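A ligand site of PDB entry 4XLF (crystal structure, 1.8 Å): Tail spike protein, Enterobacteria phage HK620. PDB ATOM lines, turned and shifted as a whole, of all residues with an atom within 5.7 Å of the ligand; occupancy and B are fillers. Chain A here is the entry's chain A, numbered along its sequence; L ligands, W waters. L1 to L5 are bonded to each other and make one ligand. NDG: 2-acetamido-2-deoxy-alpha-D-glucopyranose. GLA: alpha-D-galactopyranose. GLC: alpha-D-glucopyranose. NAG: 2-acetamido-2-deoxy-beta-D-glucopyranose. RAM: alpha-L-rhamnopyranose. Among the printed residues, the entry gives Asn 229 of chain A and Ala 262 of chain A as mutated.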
ATOM      1  N   GLY A 101     -14.906  16.438  -4.139  1.00  0.00           N
ATOM      2  CA  GLY A 101     -14.411  15.895  -5.403  1.00  0.00           C
ATOM      3  C   GLY A 101     -13.351  14.805  -5.212  1.00  0.00           C
ATOM      4  O   GLY A 101     -13.007  14.109  -6.172  1.00  0.00           O
ATOM      5  N   HIS A 102     -12.825  14.650  -4.007  1.00  0.00           N
ATOM      6  CA  HIS A 102     -11.816  13.675  -3.696  1.00  0.00           C
ATOM      7  C   HIS A 102     -12.330  12.643  -2.708  1.00  0.00           C
ATOM      8  O   HIS A 102     -11.545  11.940  -2.102  1.00  0.00           O
ATOM      9  CB  HIS A 102     -10.606  14.359  -3.101  1.00  0.00           C
ATOM     10  CG  HIS A 102     -10.097  15.504  -3.907  1.00  0.00           C
ATOM     11  ND1 HIS A 102      -9.070  15.373  -4.798  1.00  0.00           N
ATOM     12  CD2 HIS A 102     -10.424  16.799  -3.899  1.00  0.00           C
ATOM     13  CE1 HIS A 102      -8.754  16.547  -5.298  1.00  0.00           C
ATOM     14  NE2 HIS A 102      -9.592  17.441  -4.789  1.00  0.00           N
ATOM     15  N   SER A 103     -13.660  12.512  -2.619  1.00  0.00           N
ATOM     16  CA  SER A 103     -14.275  11.581  -1.597  1.00  0.00           C
ATOM     17  C   SER A 103     -13.691  11.845  -0.223  1.00  0.00           C
ATOM     18  O   SER A 103     -13.568  10.935   0.569  1.00  0.00           O
ATOM     19  CB  SER A 103     -14.078  10.139  -1.973  1.00  0.00           C
ATOM     20  OG  SER A 103     -14.425   9.945  -3.336  1.00  0.00           O
ATOM     21  N   GLN A 132     -11.122   9.401   1.082  1.00  0.00           N
ATOM     22  CA  GLN A 132      -9.762   9.878   1.345  1.00  0.00           C
ATOM     23  C   GLN A 132      -9.830  10.598   2.606  1.00  0.00           C
ATOM     24  O   GLN A 132     -10.531  11.629   2.729  1.00  0.00           O
ATOM     25  CB  GLN A 132      -9.283  10.781   0.240  1.00  0.00           C
ATOM     26  CG  GLN A 132      -9.117  10.016  -1.081  1.00  0.00           C
ATOM     27  CD  GLN A 132      -8.312  10.806  -2.116  1.00  0.00           C
ATOM     28  OE1 GLN A 132      -7.119  11.162  -1.917  1.00  0.00           O
ATOM     29  NE2 GLN A 132      -8.904  10.983  -3.275  1.00  0.00           N
ATOM     30  N   PHE A 137      -6.184  19.315  -0.570  1.00  0.00           N
ATOM     31  CA  PHE A 137      -6.736  20.113  -1.656  1.00  0.00           C
ATOM     32  C   PHE A 137      -7.896  20.972  -1.111  1.00  0.00           C
ATOM     33  O   PHE A 137      -8.593  20.556  -0.201  1.00  0.00           O
ATOM     34  CB  PHE A 137      -7.252  19.208  -2.780  1.00  0.00           C
ATOM     35  CG  PHE A 137      -6.182  18.395  -3.510  1.00  0.00           C
ATOM     36  CD1 PHE A 137      -5.265  19.016  -4.364  1.00  0.00           C
ATOM     37  CD2 PHE A 137      -6.183  17.042  -3.407  1.00  0.00           C
ATOM     38  CE1 PHE A 137      -4.334  18.217  -5.051  1.00  0.00           C
ATOM     39  CE2 PHE A 137      -5.324  16.235  -4.097  1.00  0.00           C
ATOM     40  CZ  PHE A 137      -4.395  16.838  -4.941  1.00  0.00           C
ATOM     41  N   PRO A 142      -7.816  19.528  -8.791  1.00  0.00           N
ATOM     42  CA  PRO A 142      -6.502  19.826  -8.214  1.00  0.00           C
ATOM     43  C   PRO A 142      -5.776  20.956  -8.922  1.00  0.00           C
ATOM     44  O   PRO A 142      -5.022  21.742  -8.280  1.00  0.00           O
ATOM     45  CB  PRO A 142      -5.742  18.493  -8.303  1.00  0.00           C
ATOM     46  CG  PRO A 142      -6.536  17.584  -9.147  1.00  0.00           C
ATOM     47  CD  PRO A 142      -7.959  18.118  -9.178  1.00  0.00           C
ATOM     48  N   LEU A 172     -11.219   4.753  -5.508  1.00  0.00           N
ATOM     49  CA  LEU A 172      -9.919   5.149  -4.872  1.00  0.00           C
ATOM     50  C   LEU A 172     -10.119   5.342  -3.355  1.00  0.00           C
ATOM     51  O   LEU A 172     -11.169   5.837  -2.867  1.00  0.00           O
ATOM     52  CB  LEU A 172      -9.318   6.440  -5.487  1.00  0.00           C
ATOM     53  CG  LEU A 172      -9.135   6.465  -7.018  1.00  0.00           C
ATOM     54  CD1 LEU A 172      -8.980   7.885  -7.581  1.00  0.00           C
ATOM     55  CD2 LEU A 172      -8.014   5.578  -7.442  1.00  0.00           C
ATOM     56  N   ASN A 174      -7.616   6.500   0.182  1.00  0.00           N
ATOM     57  CA  ASN A 174      -6.356   7.124   0.650  1.00  0.00           C
ATOM     58  C   ASN A 174      -6.538   7.428   2.138  1.00  0.00           C
ATOM     59  O   ASN A 174      -7.656   7.658   2.588  1.00  0.00           O
ATOM     60  CB  ASN A 174      -6.080   8.408  -0.154  1.00  0.00           C
ATOM     61  CG  ASN A 174      -4.636   8.941  -0.037  1.00  0.00           C
ATOM     62  OD1 ASN A 174      -3.708   8.354   0.564  1.00  0.00           O
ATOM     63  ND2 ASN A 174      -4.414  10.068  -0.721  1.00  0.00           N
ATOM     64  N   THR A 197      -5.944   2.317  -1.805  1.00  0.00           N
ATOM     65  CA  THR A 197      -5.148   2.471  -2.950  1.00  0.00           C
ATOM     66  C   THR A 197      -3.731   2.979  -2.498  1.00  0.00           C
ATOM     67  O   THR A 197      -2.677   2.515  -2.972  1.00  0.00           O
ATOM     68  CB  THR A 197      -5.746   3.529  -3.872  1.00  0.00           C
ATOM     69  OG1 THR A 197      -7.118   3.222  -4.204  1.00  0.00           O
ATOM     70  CG2 THR A 197      -4.874   3.638  -5.100  1.00  0.00           C
ATOM     71  N   TRP A 198      -3.756   3.943  -1.617  1.00  0.00           N
ATOM     72  CA  TRP A 198      -2.537   4.558  -0.980  1.00  0.00           C
ATOM     73  C   TRP A 198      -2.863   4.792   0.511  1.00  0.00           C
ATOM     74  O   TRP A 198      -4.073   4.943   0.879  1.00  0.00           O
ATOM     75  CB  TRP A 198      -2.198   5.912  -1.567  1.00  0.00           C
ATOM     76  CG  TRP A 198      -2.233   6.052  -3.016  1.00  0.00           C
ATOM     77  CD1 TRP A 198      -1.303   5.640  -3.898  1.00  0.00           C
ATOM     78  CD2 TRP A 198      -3.293   6.682  -3.776  1.00  0.00           C
ATOM     79  NE1 TRP A 198      -1.695   6.006  -5.182  1.00  0.00           N
ATOM     80  CE2 TRP A 198      -2.937   6.580  -5.126  1.00  0.00           C
ATOM     81  CE3 TRP A 198      -4.501   7.283  -3.425  1.00  0.00           C
ATOM     82  CZ2 TRP A 198      -3.768   7.091  -6.160  1.00  0.00           C
ATOM     83  CZ3 TRP A 198      -5.345   7.740  -4.432  1.00  0.00           C
ATOM     84  CH2 TRP A 198      -4.935   7.669  -5.783  1.00  0.00           C
ATOM     85  N   THR A 201      -0.349  10.251   0.222  1.00  0.00           N
ATOM     86  CA  THR A 201       0.225  10.838  -0.960  1.00  0.00           C
ATOM     87  C   THR A 201       0.729  12.256  -0.740  1.00  0.00           C
ATOM     88  O   THR A 201       0.147  13.002   0.060  1.00  0.00           O
ATOM     89  CB  THR A 201      -0.789  10.941  -2.104  1.00  0.00           C
ATOM     90  OG1 THR A 201      -1.833  11.861  -1.769  1.00  0.00           O
ATOM     91  CG2 THR A 201      -1.343   9.572  -2.422  1.00  0.00           C
ATOM     92  N   LEU A 202       1.848  12.551  -1.371  1.00  0.00           N
ATOM     93  CA  LEU A 202       2.545  13.780  -1.144  1.00  0.00           C
ATOM     94  C   LEU A 202       2.556  14.501  -2.470  1.00  0.00           C
ATOM     95  O   LEU A 202       2.967  13.924  -3.494  1.00  0.00           O
ATOM     96  CB  LEU A 202       3.981  13.543  -0.729  1.00  0.00           C
ATOM     97  CG  LEU A 202       4.214  12.609   0.438  1.00  0.00           C
ATOM     98  CD1 LEU A 202       5.713  12.435   0.697  1.00  0.00           C
ATOM     99  CD2 LEU A 202       3.464  13.044   1.684  1.00  0.00           C
ATOM    100  N   GLY A 203       2.107  15.719  -2.450  1.00  0.00           N
ATOM    101  CA  GLY A 203       2.215  16.557  -3.669  1.00  0.00           C
ATOM    102  C   GLY A 203       1.173  16.228  -4.695  1.00  0.00           C
ATOM    103  O   GLY A 203       0.376  15.309  -4.532  1.00  0.00           O
ATOM    104  N   TRP A 204       1.199  16.974  -5.789  1.00  0.00           N
ATOM    105  CA  TRP A 204       0.289  16.788  -6.910  1.00  0.00           C
ATOM    106  C   TRP A 204       0.987  17.196  -8.174  1.00  0.00           C
ATOM    107  O   TRP A 204       1.242  18.389  -8.386  1.00  0.00           O
ATOM    108  CB  TRP A 204      -1.060  17.508  -6.764  1.00  0.00           C
ATOM    109  CG  TRP A 204      -1.920  17.295  -7.960  1.00  0.00           C
ATOM    110  CD1 TRP A 204      -2.557  16.147  -8.294  1.00  0.00           C
ATOM    111  CD2 TRP A 204      -2.109  18.210  -9.038  1.00  0.00           C
ATOM    112  NE1 TRP A 204      -3.178  16.287  -9.519  1.00  0.00           N
ATOM    113  CE2 TRP A 204      -2.930  17.546 -10.004  1.00  0.00           C
ATOM    114  CE3 TRP A 204      -1.693  19.515  -9.296  1.00  0.00           C
ATOM    115  CZ2 TRP A 204      -3.323  18.148 -11.156  1.00  0.00           C
ATOM    116  CZ3 TRP A 204      -2.092  20.129 -10.448  1.00  0.00           C
ATOM    117  CH2 TRP A 204      -2.914  19.448 -11.386  1.00  0.00           C
ATOM    118  N   ASN A 205       1.274  16.194  -9.006  1.00  0.00           N
ATOM    119  CA  ASN A 205       1.869  16.363 -10.326  1.00  0.00           C
ATOM    120  C   ASN A 205       2.995  17.350 -10.355  1.00  0.00           C
ATOM    121  O   ASN A 205       3.024  18.237 -11.185  1.00  0.00           O
ATOM    122  CB  ASN A 205       0.824  16.698 -11.367  1.00  0.00           C
ATOM    123  CG  ASN A 205      -0.127  15.572 -11.650  1.00  0.00           C
ATOM    124  OD1 ASN A 205      -0.032  14.468 -11.078  1.00  0.00           O
ATOM    125  ND2 ASN A 205      -1.130  15.869 -12.481  1.00  0.00           N
ATOM    126  N   ASN A 229      -4.965  -1.940  -7.302  1.00  0.00           N
ATOM    127  CA  ASN A 229      -3.587  -1.416  -7.322  1.00  0.00           C
ATOM    128  C   ASN A 229      -3.363  -0.711  -6.047  1.00  0.00           C
ATOM    129  O   ASN A 229      -4.284  -0.048  -5.519  1.00  0.00           O
ATOM    130  CB  ASN A 229      -3.417  -0.447  -8.494  1.00  0.00           C
ATOM    131  CG  ASN A 229      -1.983  -0.279  -8.945  1.00  0.00           C
ATOM    132  OD1 ASN A 229      -1.003  -0.485  -8.200  1.00  0.00           O
ATOM    133  ND2 ASN A 229      -1.851   0.146 -10.181  1.00  0.00           N
ATOM    134  N   HIS A 230      -2.154  -0.854  -5.528  1.00  0.00           N
ATOM    135  CA  HIS A 230      -1.797  -0.213  -4.281  1.00  0.00           C
ATOM    136  C   HIS A 230      -0.359   0.239  -4.239  1.00  0.00           C
ATOM    137  O   HIS A 230       0.498  -0.530  -4.660  1.00  0.00           O
ATOM    138  CB  HIS A 230      -2.008  -1.167  -3.129  1.00  0.00           C
ATOM    139  CG  HIS A 230      -1.578  -0.610  -1.798  1.00  0.00           C
ATOM    140  ND1 HIS A 230      -2.464  -0.082  -0.876  1.00  0.00           N
ATOM    141  CD2 HIS A 230      -0.357  -0.560  -1.215  1.00  0.00           C
ATOM    142  CE1 HIS A 230      -1.801   0.273   0.199  1.00  0.00           C
ATOM    143  NE2 HIS A 230      -0.525  -0.013   0.022  1.00  0.00           N
ATOM    144  N   SER A 231      -0.150   1.474  -3.820  1.00  0.00           N
ATOM    145  CA  SER A 231       1.189   2.053  -3.510  1.00  0.00           C
ATOM    146  C   SER A 231       1.070   2.782  -2.165  1.00  0.00           C
ATOM    147  O   SER A 231       0.339   3.739  -2.050  1.00  0.00           O
ATOM    148  CB  SER A 231       1.704   2.999  -4.579  1.00  0.00           C
ATOM    149  OG  SER A 231       3.027   3.369  -4.246  1.00  0.00           O
ATOM    150  N   TYR A 234       2.805   7.543  -2.179  1.00  0.00           N
ATOM    151  CA  TYR A 234       3.110   8.087  -3.484  1.00  0.00           C
ATOM    152  C   TYR A 234       3.722   9.498  -3.374  1.00  0.00           C
ATOM    153  O   TYR A 234       3.101  10.395  -2.811  1.00  0.00           O
ATOM    154  CB  TYR A 234       1.831   8.087  -4.315  1.00  0.00           C
ATOM    155  CG  TYR A 234       1.881   8.131  -5.832  1.00  0.00           C
ATOM    156  CD1 TYR A 234       2.240   9.278  -6.521  1.00  0.00           C
ATOM    157  CD2 TYR A 234       1.450   7.046  -6.590  1.00  0.00           C
ATOM    158  CE1 TYR A 234       2.230   9.310  -7.932  1.00  0.00           C
ATOM    159  CE2 TYR A 234       1.437   7.105  -7.975  1.00  0.00           C
ATOM    160  CZ  TYR A 234       1.794   8.227  -8.648  1.00  0.00           C
ATOM    161  OH  TYR A 234       1.704   8.292 -10.036  1.00  0.00           O
ATOM    162  N   ASN A 236       4.802  12.671  -5.077  1.00  0.00           N
ATOM    163  CA  ASN A 236       4.554  13.388  -6.310  1.00  0.00           C
ATOM    164  C   ASN A 236       4.911  14.876  -6.206  1.00  0.00           C
ATOM    165  O   ASN A 236       4.351  15.712  -6.872  1.00  0.00           O
ATOM    166  CB  ASN A 236       3.100  13.216  -6.721  1.00  0.00           C
ATOM    167  CG  ASN A 236       2.905  13.240  -8.245  1.00  0.00           C
ATOM    168  OD1 ASN A 236       3.839  13.411  -8.985  1.00  0.00           O
ATOM    169  ND2 ASN A 236       1.647  13.106  -8.664  1.00  0.00           N
ATOM    170  N   ALA A 262       6.199   4.929  -4.300  1.00  0.00           N
ATOM    171  CA  ALA A 262       6.423   5.402  -5.635  1.00  0.00           C
ATOM    172  C   ALA A 262       7.196   6.729  -5.527  1.00  0.00           C
ATOM    173  O   ALA A 262       6.676   7.692  -4.959  1.00  0.00           O
ATOM    174  CB  ALA A 262       5.114   5.652  -6.374  1.00  0.00           C
ATOM    175  N   HIS A 264       8.228   9.775  -7.705  1.00  0.00           N
ATOM    176  CA  HIS A 264       7.835  10.259  -9.010  1.00  0.00           C
ATOM    177  C   HIS A 264       8.224  11.692  -9.369  1.00  0.00           C
ATOM    178  O   HIS A 264       7.724  12.228 -10.376  1.00  0.00           O
ATOM    179  CB  HIS A 264       6.303  10.102  -9.180  1.00  0.00           C
ATOM    180  CG  HIS A 264       5.837   8.741  -9.606  1.00  0.00           C
ATOM    181  ND1 HIS A 264       4.727   8.587 -10.397  1.00  0.00           N
ATOM    182  CD2 HIS A 264       6.283   7.499  -9.361  1.00  0.00           C
ATOM    183  CE1 HIS A 264       4.502   7.306 -10.627  1.00  0.00           C
ATOM    184  NE2 HIS A 264       5.386   6.616  -9.949  1.00  0.00           N
ATOM    185  N   TYR A 283       8.589   1.988  -7.004  1.00  0.00           N
ATOM    186  CA  TYR A 283       8.667   2.563  -8.366  1.00  0.00           C
ATOM    187  C   TYR A 283       9.525   3.872  -8.350  1.00  0.00           C
ATOM    188  O   TYR A 283       9.378   4.716  -7.489  1.00  0.00           O
ATOM    189  CB  TYR A 283       7.281   2.892  -8.968  1.00  0.00           C
ATOM    190  CG  TYR A 283       6.505   1.665  -9.354  1.00  0.00           C
ATOM    191  CD1 TYR A 283       6.662   1.100 -10.620  1.00  0.00           C
ATOM    192  CD2 TYR A 283       5.611   1.044  -8.477  1.00  0.00           C
ATOM    193  CE1 TYR A 283       5.947  -0.032 -10.996  1.00  0.00           C
ATOM    194  CE2 TYR A 283       4.914  -0.048  -8.863  1.00  0.00           C
ATOM    195  CZ  TYR A 283       5.075  -0.590 -10.111  1.00  0.00           C
ATOM    196  OH  TYR A 283       4.375  -1.726 -10.454  1.00  0.00           O
ATOM    197  N   VAL A 285       9.967   6.596 -11.257  1.00  0.00           N
ATOM    198  CA  VAL A 285       9.328   6.751 -12.572  1.00  0.00           C
ATOM    199  C   VAL A 285       9.116   8.223 -12.796  1.00  0.00           C
ATOM    200  O   VAL A 285       8.746   8.948 -11.850  1.00  0.00           O
ATOM    201  CB  VAL A 285       7.985   5.999 -12.592  1.00  0.00           C
ATOM    202  CG1 VAL A 285       7.197   6.291 -13.914  1.00  0.00           C
ATOM    203  CG2 VAL A 285       8.195   4.487 -12.452  1.00  0.00           C
ATOM    204  N   HIS A 287       6.454  10.030 -14.966  1.00  0.00           N
ATOM    205  CA  HIS A 287       5.285  10.083 -15.852  1.00  0.00           C
ATOM    206  C   HIS A 287       5.176  11.481 -16.502  1.00  0.00           C
ATOM    207  O   HIS A 287       5.059  12.527 -15.785  1.00  0.00           O
ATOM    208  CB  HIS A 287       4.006   9.876 -15.081  1.00  0.00           C
ATOM    209  CG  HIS A 287       3.723   8.468 -14.667  1.00  0.00           C
ATOM    210  ND1 HIS A 287       3.995   7.361 -15.424  1.00  0.00           N
ATOM    211  CD2 HIS A 287       3.123   7.991 -13.540  1.00  0.00           C
ATOM    212  CE1 HIS A 287       3.596   6.271 -14.799  1.00  0.00           C
ATOM    213  NE2 HIS A 287       3.117   6.620 -13.618  1.00  0.00           N
ATOM    214  N   ALA A 289       2.672  12.604 -17.741  1.00  0.00           N
ATOM    215  CA  ALA A 289       1.420  13.117 -17.213  1.00  0.00           C
ATOM    216  C   ALA A 289       1.477  13.839 -15.895  1.00  0.00           C
ATOM    217  O   ALA A 289       0.482  14.474 -15.499  1.00  0.00           O
ATOM    218  CB  ALA A 289       0.422  11.952 -17.092  1.00  0.00           C
ATOM    219  N   GLU A 290       2.578  13.700 -15.156  1.00  0.00           N
ATOM    220  CA  GLU A 290       2.715  14.275 -13.874  1.00  0.00           C
ATOM    221  C   GLU A 290       3.763  15.381 -13.875  1.00  0.00           C
ATOM    222  O   GLU A 290       4.222  15.775 -12.840  1.00  0.00           O
ATOM    223  CB  GLU A 290       3.098  13.155 -12.854  1.00  0.00           C
ATOM    224  CG  GLU A 290       1.992  12.114 -12.736  1.00  0.00           C
ATOM    225  CD  GLU A 290       2.282  11.054 -11.707  1.00  0.00           C
ATOM    226  OE1 GLU A 290       3.482  10.768 -11.458  1.00  0.00           O
ATOM    227  OE2 GLU A 290       1.340  10.479 -11.161  1.00  0.00           O
ATOM    228  N   ASN A 361       2.566   2.196 -18.695  1.00  0.00           N
ATOM    229  CA  ASN A 361       1.303   1.608 -18.268  1.00  0.00           C
ATOM    230  C   ASN A 361       0.464   1.006 -19.403  1.00  0.00           C
ATOM    231  O   ASN A 361      -0.332   0.163 -19.137  1.00  0.00           O
ATOM    232  CB  ASN A 361       0.443   2.596 -17.439  1.00  0.00           C
ATOM    233  CG  ASN A 361       1.024   2.828 -16.061  1.00  0.00           C
ATOM    234  OD1 ASN A 361       1.903   2.096 -15.641  1.00  0.00           O
ATOM    235  ND2 ASN A 361       0.547   3.851 -15.352  1.00  0.00           N
HETATM  236  C1  NDG L   1       1.858   1.951  -9.676  1.00  0.00           C
HETATM  237  C2  NDG L   1       0.950   3.160  -9.427  1.00  0.00           C
HETATM  238  C3  NDG L   1       0.542   3.788 -10.768  1.00  0.00           C
HETATM  239  C4  NDG L   1       1.846   4.144 -11.542  1.00  0.00           C
HETATM  240  C5  NDG L   1       2.854   2.944 -11.669  1.00  0.00           C
HETATM  241  C6  NDG L   1       4.286   3.431 -12.064  1.00  0.00           C
HETATM  242  C7  NDG L   1      -0.648   3.389  -7.581  1.00  0.00           C
HETATM  243  C8  NDG L   1      -1.730   2.727  -6.814  1.00  0.00           C
HETATM  244  O5  NDG L   1       3.011   2.285 -10.410  1.00  0.00           O
HETATM  245  O3  NDG L   1      -0.267   4.961 -10.583  1.00  0.00           O
HETATM  246  O4  NDG L   1       1.592   4.664 -12.846  1.00  0.00           O
HETATM  247  O6  NDG L   1       4.858   3.936 -10.778  1.00  0.00           O
HETATM  248  O7  NDG L   1      -0.248   4.548  -7.298  1.00  0.00           O
HETATM  249  N2  NDG L   1      -0.145   2.674  -8.607  1.00  0.00           N
HETATM  250  O1  NDG L   1       1.137   0.982 -10.360  1.00  0.00           O
HETATM  251  C1  GLA L   2      -1.229   5.146 -11.626  1.00  0.00           C
HETATM  252  C2  GLA L   2      -1.538   6.647 -11.589  1.00  0.00           C
HETATM  253  C3  GLA L   2      -2.188   7.039 -10.229  1.00  0.00           C
HETATM  254  C4  GLA L   2      -3.365   6.143  -9.907  1.00  0.00           C
HETATM  255  C5  GLA L   2      -2.911   4.675  -9.967  1.00  0.00           C
HETATM  256  C6  GLA L   2      -4.008   3.652  -9.745  1.00  0.00           C
HETATM  257  O2  GLA L   2      -0.323   7.369 -11.767  1.00  0.00           O
HETATM  258  O3  GLA L   2      -2.593   8.396 -10.358  1.00  0.00           O
HETATM  259  O4  GLA L   2      -4.423   6.336 -10.893  1.00  0.00           O
HETATM  260  O5  GLA L   2      -2.352   4.394 -11.275  1.00  0.00           O
HETATM  261  O6  GLA L   2      -4.662   3.882  -8.494  1.00  0.00           O
HETATM  262  C1  GLC L   3      -5.705   6.551 -10.279  1.00  0.00           C
HETATM  263  C2  GLC L   3      -6.781   6.514 -11.372  1.00  0.00           C
HETATM  264  C3  GLC L   3      -6.671   7.732 -12.323  1.00  0.00           C
HETATM  265  C4  GLC L   3      -6.787   8.968 -11.472  1.00  0.00           C
HETATM  266  C5  GLC L   3      -5.639   8.970 -10.425  1.00  0.00           C
HETATM  267  C6  GLC L   3      -5.611  10.165  -9.468  1.00  0.00           C
HETATM  268  O2  GLC L   3      -6.611   5.324 -12.124  1.00  0.00           O
HETATM  269  O3  GLC L   3      -7.786   7.629 -13.203  1.00  0.00           O
HETATM  270  O4  GLC L   3      -6.683  10.080 -12.307  1.00  0.00           O
HETATM  271  O5  GLC L   3      -5.788   7.785  -9.598  1.00  0.00           O
HETATM  272  O6  GLC L   3      -6.915  10.237  -8.822  1.00  0.00           O
HETATM  273  C1  NAG L   4      -1.769   9.302  -9.591  1.00  0.00           C
HETATM  274  C2  NAG L   4      -2.032  10.667 -10.259  1.00  0.00           C
HETATM  275  C3  NAG L   4      -1.373  11.784  -9.459  1.00  0.00           C
HETATM  276  C4  NAG L   4      -1.538  11.676  -7.946  1.00  0.00           C
HETATM  277  C5  NAG L   4      -1.234  10.289  -7.536  1.00  0.00           C
HETATM  278  C6  NAG L   4      -1.520  10.036  -6.102  1.00  0.00           C
HETATM  279  C7  NAG L   4      -2.221  10.677 -12.677  1.00  0.00           C
HETATM  280  C8  NAG L   4      -1.541  10.465 -13.991  1.00  0.00           C
HETATM  281  N2  NAG L   4      -1.486  10.537 -11.591  1.00  0.00           N
HETATM  282  O3  NAG L   4      -1.921  13.002  -9.926  1.00  0.00           O
HETATM  283  O4  NAG L   4      -0.630  12.602  -7.268  1.00  0.00           O
HETATM  284  O5  NAG L   4      -2.067   9.395  -8.209  1.00  0.00           O
HETATM  285  O6  NAG L   4      -2.854  10.280  -5.734  1.00  0.00           O
HETATM  286  O7  NAG L   4      -3.414  11.003 -12.634  1.00  0.00           O
HETATM  287  C1  RAM L   5      -7.534  11.480  -9.221  1.00  0.00           C
HETATM  288  C2  RAM L   5      -8.907  11.497  -8.559  1.00  0.00           C
HETATM  289  C3  RAM L   5      -8.791  11.737  -7.094  1.00  0.00           C
HETATM  290  C4  RAM L   5      -7.894  12.938  -6.792  1.00  0.00           C
HETATM  291  C5  RAM L   5      -6.565  12.725  -7.454  1.00  0.00           C
HETATM  292  C6  RAM L   5      -5.673  13.980  -7.368  1.00  0.00           C
HETATM  293  O2  RAM L   5      -9.650  12.565  -9.160  1.00  0.00           O
HETATM  294  O3  RAM L   5     -10.140  12.008  -6.648  1.00  0.00           O
HETATM  295  O4  RAM L   5      -7.821  13.070  -5.356  1.00  0.00           O
HETATM  296  O5  RAM L   5      -6.770  12.612  -8.876  1.00  0.00           O
HETATM  297  O   HOH W   1      -9.376   4.400 -11.051  1.00  0.00           O
HETATM  298  O   HOH W   2      -4.630  13.954 -10.651  1.00  0.00           O
HETATM  299  O   HOH W   3     -11.603   9.821  -5.042  1.00  0.00           O
HETATM  300  O   HOH W   4      -5.883  12.832  -3.587  1.00  0.00           O
HETATM  301  O   HOH W   5      -7.904   9.123 -15.637  1.00  0.00           O
HETATM  302  O   HOH W   6       1.725  -1.586 -10.330  1.00  0.00           O
HETATM  303  O   HOH W   7      -0.242   7.157 -14.640  1.00  0.00           O
HETATM  304  O   HOH W   8      -3.286  13.952 -13.171  1.00  0.00           O
HETATM  305  O   HOH W   9      -4.284   4.603 -13.394  1.00  0.00           O
HETATM  306  O   HOH W  10      -3.326  12.309  -3.939  1.00  0.00           O
HETATM  307  O   HOH W  11      -1.910  14.179  -5.604  1.00  0.00           O
HETATM  308  O   HOH W  12      -8.368   5.593 -14.693  1.00  0.00           O
HETATM  309  O   HOH W  13     -12.528  11.666  -7.605  1.00  0.00           O
HETATM  310  O   HOH W  14       0.998  11.880  -4.647  1.00  0.00           O
HETATM  311  O   HOH W  15      -6.387   1.937  -8.145  1.00  0.00           O
HETATM  312  O   HOH W  16     -10.309   7.139 -12.919  1.00  0.00           O
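ND1 of His 264 is in hydrogen-bond range of OE1 of Glu 290, at 2.7 Å.
The side-chain hydroxyl of Tyr 234 lies close to a ring nitrogen (ND1) of His 264 (3.1 Å).
O of Thr 197 lies close to ND1 of His 230, at 3.3 Å.
The side-chain amide nitrogen (NE2) of Gln 132 lies within hydrogen-bond range of the backbone carbonyl oxygen (O) of His 102, at 3.0 Å.
The backbone NH (N) of Gln 132 sits at hydrogen-bond distance from the backbone carbonyl oxygen (O) of Ser 103, at 2.9 Å.
The side-chain amide oxygen (OD1) of Asn 174 sits close to the backbone carbonyl oxygen (O) of Trp 198 (3.4 Å).
The side-chain hydroxyl (OH) of Tyr 234 lies within hydrogen-bond range of the side-chain carboxylate (OE2) of Glu 290 (2.5 Å).
The backbone NH (N) of Asn 236 is in hydrogen-bond range of the backbone carbonyl oxygen (O) of Leu 202, at 2.7 Å.
Water W13 bridges an oxygen (O3) of RAM L5 and the backbone carbonyl oxygen of Gly 101.
Water W11 lies within hydrogen-bond range of O4 of NAG L4 (2.6 Å) and O of Gly 203 (2.8 Å).
Water W4 bridges O4 of RAM L5 (2.6 Å) and OE1 of Gln 132 (2.7 Å).
Water W7 lies within hydrogen-bond range of an oxygen (O2) of GLA L2 (2.9 Å) and the side-chain amide nitrogen of Asn 361 (3.5 Å).
Water W8 bridges ND2 of Asn 205 (3.0 Å) and O7 of NAG L4 (3.0 Å).
Water W3 lies within hydrogen-bond range of an oxygen (O3) of RAM L5 (3.1 Å), the side-chain hydroxyl of Ser 103 (3.3 Å) and the side-chain amide nitrogen of Gln 132 (3.4 Å).
An oxygen (O7) of NDG L1 sits at hydrogen-bond distance from the indole nitrogen (NE1) of Trp 198.
An oxygen (O6) of NDG L1 sits at hydrogen-bond distance from a ring nitrogen (NE2) of His 264, 2.9 Å away.
NE2 of His 287 is in hydrogen-bond range of O4 of NDG L1, at 2.6 Å.
A ring nitrogen (ND1) of His 102 is in hydrogen-bond range of an oxygen (O4) of RAM L5, 2.7 Å away.
O2 of GLA L2 is in hydrogen-bond range of OH of Tyr 234.
ND2 of Asn 229 sits at hydrogen-bond distance from O1 of NDG L1, at 3.1 Å.
The side-chain amide nitrogen (NE2) of Gln 132 is in hydrogen-bond range of an oxygen (O4) of RAM L5, 3.1 Å away.
An oxygen (O4) of NDG L1 is in hydrogen-bond range of the side-chain amide nitrogen (ND2) of Asn 361 (2.8 Å).
An oxygen (O4) of NAG L4 sits at hydrogen-bond distance from the side-chain amide nitrogen (ND2) of Asn 236, 2.7 Å away.
The side-chain amide oxygen (OD1) of Asn 205 is in hydrogen-bond range of an oxygen (O3) of NAG L4 (2.7 Å).
The side-chain carboxylate of Glu 290 lies within hydrogen-bond range of a nitrogen (N2) of NAG L4 (2.9 Å).
O of Gly 101 touches O3 of RAM L5, 3.6 Å away.
Phe 137 touches the ligand.
CD1 of Leu 172 touches O6 of GLC L3 (3.4 Å).
CG2 of Thr 197 touches O6 of GLA L2, at 3.4 Å.
CG2 of Thr 201 touches O6 of NAG L4, 3.7 Å away.
Gly 203 touches the ligand.
NE1 of Trp 204 touches O3 of NAG L4 (3.5 Å).
His 230 touches the ligand.
N of Ser 231 touches C8 of NDG L1, at 3.6 Å.
CG of Tyr 283 touches O6 of NDG L1 (3.1 Å).
CG2 of Val 285 touches O6 of NDG L1 (3.8 Å).
Ala 289 touches the ligand.
Hydrophobic or aromatic side chains within 4 Å of the ligand: His 102, Phe 137, Leu 172, Trp 198, Trp 204, Tyr 234, His 264, Tyr 283, Val 285, His 287 and Ala 289.
23 residues have an atom within 4 Å of the ligand: Gly 101, His 102, Gln 132, Phe 137, Leu 172, Thr 197, Trp 198, Thr 201, Gly 203, Trp 204, Asn 205, Asn 229, His 230, Ser 231, Tyr 234, Asn 236, His 264, Tyr 283, Val 285, His 287, Ala 289, Glu 290 and Asn 361.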
